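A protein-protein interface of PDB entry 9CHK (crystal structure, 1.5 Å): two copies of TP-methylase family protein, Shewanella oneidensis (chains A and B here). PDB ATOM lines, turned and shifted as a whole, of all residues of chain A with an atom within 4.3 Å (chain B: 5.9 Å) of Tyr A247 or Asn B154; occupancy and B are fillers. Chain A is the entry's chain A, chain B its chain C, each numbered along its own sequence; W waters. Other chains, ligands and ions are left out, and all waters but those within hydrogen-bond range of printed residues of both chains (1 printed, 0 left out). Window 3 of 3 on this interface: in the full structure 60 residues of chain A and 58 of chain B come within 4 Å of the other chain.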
ATOM      1  N   GLU A 246      20.677   7.713  12.961  1.00  0.00           N
ATOM      2  CA  GLU A 246      22.045   7.720  12.465  1.00  0.00           C
ATOM      3  C   GLU A 246      22.376   9.103  11.909  1.00  0.00           C
ATOM      4  O   GLU A 246      21.505   9.787  11.372  1.00  0.00           O
ATOM      5  CB  GLU A 246      22.238   6.679  11.364  1.00  0.00           C
ATOM      6  CG  GLU A 246      22.054   5.242  11.842  1.00  0.00           C
ATOM      7  CD  GLU A 246      22.229   4.225  10.731  1.00  0.00           C
ATOM      8  OE1 GLU A 246      23.377   4.054  10.271  1.00  0.00           O
ATOM      9  OE2 GLU A 246      21.218   3.625  10.311  1.00  0.00           O
ATOM     10  N   TYR A 247      23.649   9.493  12.018  1.00  0.00           N
ATOM     11  CA  TYR A 247      24.068  10.833  11.647  1.00  0.00           C
ATOM     12  C   TYR A 247      24.034  10.987  10.130  1.00  0.00           C
ATOM     13  O   TYR A 247      24.480  10.115   9.384  1.00  0.00           O
ATOM     14  CB  TYR A 247      25.461  11.180  12.185  1.00  0.00           C
ATOM     15  CG  TYR A 247      25.536  11.255  13.703  1.00  0.00           C
ATOM     16  CD1 TYR A 247      24.966  12.316  14.397  1.00  0.00           C
ATOM     17  CD2 TYR A 247      26.174  10.265  14.441  1.00  0.00           C
ATOM     18  CE1 TYR A 247      25.033  12.392  15.779  1.00  0.00           C
ATOM     19  CE2 TYR A 247      26.246  10.330  15.823  1.00  0.00           C
ATOM     20  CZ  TYR A 247      25.674  11.396  16.493  1.00  0.00           C
ATOM     21  OH  TYR A 247      25.745  11.458  17.855  1.00  0.00           O
ATOM     22  N   ASN A 248      23.509  12.138   9.705  1.00  0.00           N
ATOM     23  CA  ASN A 248      23.477  12.536   8.311  1.00  0.00           C
ATOM     24  C   ASN A 248      24.780  13.264   7.985  1.00  0.00           C
ATOM     25  O   ASN A 248      24.815  14.490   7.938  1.00  0.00           O
ATOM     26  CB  ASN A 248      22.273  13.434   8.056  1.00  0.00           C
ATOM     27  CG  ASN A 248      21.895  13.502   6.599  1.00  0.00           C
ATOM     28  OD1 ASN A 248      22.772  13.497   5.729  1.00  0.00           O
ATOM     29  ND2 ASN A 248      20.599  13.545   6.317  1.00  0.00           N
ATOM     30  N   TYR A 249      25.854  12.500   7.762  1.00  0.00           N
ATOM     31  CA  TYR A 249      27.192  13.068   7.691  1.00  0.00           C
ATOM     32  C   TYR A 249      27.303  14.100   6.574  1.00  0.00           C
ATOM     33  O   TYR A 249      27.980  15.114   6.736  1.00  0.00           O
ATOM     34  CB  TYR A 249      28.245  11.975   7.504  1.00  0.00           C
ATOM     35  CG  TYR A 249      28.504  11.188   8.779  1.00  0.00           C
ATOM     36  CD1 TYR A 249      29.099  11.797   9.876  1.00  0.00           C
ATOM     37  CD2 TYR A 249      28.157   9.846   8.888  1.00  0.00           C
ATOM     38  CE1 TYR A 249      29.339  11.099  11.045  1.00  0.00           C
ATOM     39  CE2 TYR A 249      28.396   9.134  10.052  1.00  0.00           C
ATOM     40  CZ  TYR A 249      28.986   9.764  11.133  1.00  0.00           C
ATOM     41  OH  TYR A 249      29.236   9.080  12.286  1.00  0.00           O
ATOM     42  N   LEU A 252      25.679  17.271   7.882  1.00  0.00           N
ATOM     43  CA  LEU A 252      26.445  17.784   9.007  1.00  0.00           C
ATOM     44  C   LEU A 252      27.697  18.487   8.490  1.00  0.00           C
ATOM     45  O   LEU A 252      28.051  19.569   8.956  1.00  0.00           O
ATOM     46  CB  LEU A 252      26.797  16.662   9.982  1.00  0.00           C
ATOM     47  CG  LEU A 252      25.621  16.049  10.750  1.00  0.00           C
ATOM     48  CD1 LEU A 252      26.093  14.902  11.631  1.00  0.00           C
ATOM     49  CD2 LEU A 252      24.880  17.086  11.577  1.00  0.00           C
ATOM     50  N   PRO A 259      28.718  15.232  15.438  1.00  0.00           N
ATOM     51  CA  PRO A 259      28.043  14.703  16.625  1.00  0.00           C
ATOM     52  C   PRO A 259      28.294  15.512  17.896  1.00  0.00           C
ATOM     53  O   PRO A 259      27.378  15.728  18.686  1.00  0.00           O
ATOM     54  CB  PRO A 259      28.624  13.282  16.703  1.00  0.00           C
ATOM     55  CG  PRO A 259      28.826  12.901  15.255  1.00  0.00           C
ATOM     56  CD  PRO A 259      29.345  14.181  14.618  1.00  0.00           C
ATOM     57  N   GLN B 149      16.256  18.019  13.211  1.00  0.00           N
ATOM     58  CA  GLN B 149      16.497  16.594  13.346  1.00  0.00           C
ATOM     59  C   GLN B 149      16.498  15.939  11.965  1.00  0.00           C
ATOM     60  O   GLN B 149      17.252  15.001  11.717  1.00  0.00           O
ATOM     61  CB  GLN B 149      15.453  15.947  14.249  1.00  0.00           C
ATOM     62  CG  GLN B 149      15.748  14.482  14.531  1.00  0.00           C
ATOM     63  CD  GLN B 149      14.684  13.838  15.387  1.00  0.00           C
ATOM     64  OE1 GLN B 149      13.786  13.152  14.886  1.00  0.00           O
ATOM     65  NE2 GLN B 149      14.755  14.094  16.685  1.00  0.00           N
ATOM     66  N   PHE B 150      15.656  16.463  11.068  1.00  0.00           N
ATOM     67  CA  PHE B 150      15.561  15.970   9.704  1.00  0.00           C
ATOM     68  C   PHE B 150      16.899  16.176   8.998  1.00  0.00           C
ATOM     69  O   PHE B 150      17.293  15.364   8.164  1.00  0.00           O
ATOM     70  CB  PHE B 150      14.406  16.665   8.970  1.00  0.00           C
ATOM     71  CG  PHE B 150      14.125  16.109   7.581  1.00  0.00           C
ATOM     72  CD1 PHE B 150      13.259  15.036   7.406  1.00  0.00           C
ATOM     73  CD2 PHE B 150      14.740  16.649   6.454  1.00  0.00           C
ATOM     74  CE1 PHE B 150      13.009  14.524   6.143  1.00  0.00           C
ATOM     75  CE2 PHE B 150      14.485  16.133   5.191  1.00  0.00           C
ATOM     76  CZ  PHE B 150      13.619  15.072   5.039  1.00  0.00           C
ATOM     77  N   PHE B 152      19.986  16.661  10.649  1.00  0.00           N
ATOM     78  CA  PHE B 152      21.138  16.137  11.372  1.00  0.00           C
ATOM     79  C   PHE B 152      21.199  14.613  11.286  1.00  0.00           C
ATOM     80  O   PHE B 152      22.276  14.029  11.410  1.00  0.00           O
ATOM     81  CB  PHE B 152      21.122  16.528  12.854  1.00  0.00           C
ATOM     82  CG  PHE B 152      21.165  18.019  13.156  1.00  0.00           C
ATOM     83  CD1 PHE B 152      21.624  18.935  12.217  1.00  0.00           C
ATOM     84  CD2 PHE B 152      20.750  18.500  14.394  1.00  0.00           C
ATOM     85  CE1 PHE B 152      21.663  20.291  12.509  1.00  0.00           C
ATOM     86  CE2 PHE B 152      20.788  19.855  14.679  1.00  0.00           C
ATOM     87  CZ  PHE B 152      21.245  20.747  13.737  1.00  0.00           C
ATOM     88  N   PHE B 153      20.038  13.977  11.108  1.00  0.00           N
ATOM     89  CA  PHE B 153      19.938  12.528  11.166  1.00  0.00           C
ATOM     90  C   PHE B 153      19.262  12.027   9.895  1.00  0.00           C
ATOM     91  O   PHE B 153      18.619  12.797   9.184  1.00  0.00           O
ATOM     92  CB  PHE B 153      19.180  12.112  12.431  1.00  0.00           C
ATOM     93  CG  PHE B 153      19.862  12.520  13.730  1.00  0.00           C
ATOM     94  CD1 PHE B 153      20.866  11.734  14.285  1.00  0.00           C
ATOM     95  CD2 PHE B 153      19.504  13.690  14.391  1.00  0.00           C
ATOM     96  CE1 PHE B 153      21.488  12.106  15.465  1.00  0.00           C
ATOM     97  CE2 PHE B 153      20.133  14.059  15.570  1.00  0.00           C
ATOM     98  CZ  PHE B 153      21.123  13.269  16.104  1.00  0.00           C
ATOM     99  N   ASN B 154      19.411  10.729   9.619  1.00  0.00           N
ATOM    100  CA  ASN B 154      18.853  10.142   8.412  1.00  0.00           C
ATOM    101  C   ASN B 154      17.380   9.814   8.641  1.00  0.00           C
ATOM    102  O   ASN B 154      17.043   8.776   9.198  1.00  0.00           O
ATOM    103  CB  ASN B 154      19.660   8.935   7.945  1.00  0.00           C
ATOM    104  CG  ASN B 154      21.074   9.316   7.584  1.00  0.00           C
ATOM    105  OD1 ASN B 154      21.297  10.372   6.980  1.00  0.00           O
ATOM    106  ND2 ASN B 154      22.043   8.492   7.956  1.00  0.00           N
ATOM    107  N   HIS B 155      16.515  10.738   8.214  1.00  0.00           N
ATOM    108  CA  HIS B 155      15.089  10.484   8.120  1.00  0.00           C
ATOM    109  C   HIS B 155      14.741  10.350   6.641  1.00  0.00           C
ATOM    110  O   HIS B 155      15.337  11.012   5.794  1.00  0.00           O
ATOM    111  CB  HIS B 155      14.288  11.602   8.796  1.00  0.00           C
ATOM    112  CG  HIS B 155      14.208  11.501  10.282  1.00  0.00           C
ATOM    113  ND1 HIS B 155      13.727  10.382  10.931  1.00  0.00           N
ATOM    114  CD2 HIS B 155      14.494  12.393  11.242  1.00  0.00           C
ATOM    115  CE1 HIS B 155      13.748  10.594  12.240  1.00  0.00           C
ATOM    116  NE2 HIS B 155      14.212  11.810  12.451  1.00  0.00           N
ATOM    117  N   VAL B 156      13.777   9.477   6.348  1.00  0.00           N
ATOM    118  CA  VAL B 156      13.426   9.164   4.976  1.00  0.00           C
ATOM    119  C   VAL B 156      11.942   9.445   4.789  1.00  0.00           C
ATOM    120  O   VAL B 156      11.105   8.669   5.240  1.00  0.00           O
ATOM    121  CB  VAL B 156      13.755   7.696   4.647  1.00  0.00           C
ATOM    122  CG1 VAL B 156      13.310   7.317   3.241  1.00  0.00           C
ATOM    123  CG2 VAL B 156      15.233   7.391   4.848  1.00  0.00           C
HETATM  124  O   HOH W   1      18.665   7.637  11.125  1.00  0.00           O
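Among the printed residues, merely in contact across the chains: Glu A246 with Phe B153 (3.2 Å), Asn A248 with Phe B153 (3.6 Å), Tyr A247 with Phe B153 (3.6 Å), Tyr A247 with Phe B152 (3.7 Å) and Leu A252 with Phe B152 (3.8 Å).
O of Glu A246 is in hydrogen-bond range of N of Asn B154, at 2.9 Å.
The backbone carbonyl oxygen (O) of Tyr A247 lies within hydrogen-bond range of the side-chain amide nitrogen (ND2) of Asn B154 (3.3 Å).
The backbone NH (N) of Asn A248 sits at hydrogen-bond distance from the backbone carbonyl oxygen (O) of Phe B152 (2.8 Å).
OD1 of Asn B154 lies close to ND2 of Asn A248 (3.3 Å).
Of the 6 printed residues of chain A, 4 touch a printed residue of chain B.
Printed residues of chain A that touch a printed residue of chain B: Glu A246, Tyr A247, Asn A248 and Leu A252.
Of the 7 printed residues of chain B, 3 touch a printed residue of chain A.
Water W1 lies within hydrogen-bond range of N of Glu A246 (2.7 Å) and O of Asn B154 (2.8 Å).
Of the printed residues of chain B, Glu A246 touches Phe B153 and Asn B154.
Of chain B, only Phe B152, Phe B153 and Asn B154 come within 4 Å of Tyr A247.
Of the printed residues of chain B, Asn A248 touches Phe B152 (2.8 Å), Phe B153 (3.6 Å) and Asn B154 (3.2 Å).
Printed residues of chain B within 4 Å of Leu A252: Phe B152.
Pro A259 touches none of the printed residues of chain B.
Of the printed residues of chain A, Phe B152 touches Tyr A247, Asn A248 and Leu A252.
Printed residues of chain A within 4 Å of Phe B153: Glu A246, Tyr A247 and Asn A248.
Asn B154 touches just these residues of chain A: Glu A246 (2.9 Å), Tyr A247 (3.3 Å) and Asn A248 (3.2 Å).
The nearest printed residue of chain B that does not touch Tyr A247 is His B155 (7.8 Å).
The nearest printed residue of chain B that does not touch Asn A248 is Phe B150 (4.2 Å).
No position is printed for both chains.
Of the 9 pairs that touch across the chains among the printed residues, none has its exchanged pair printed and touching as well.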
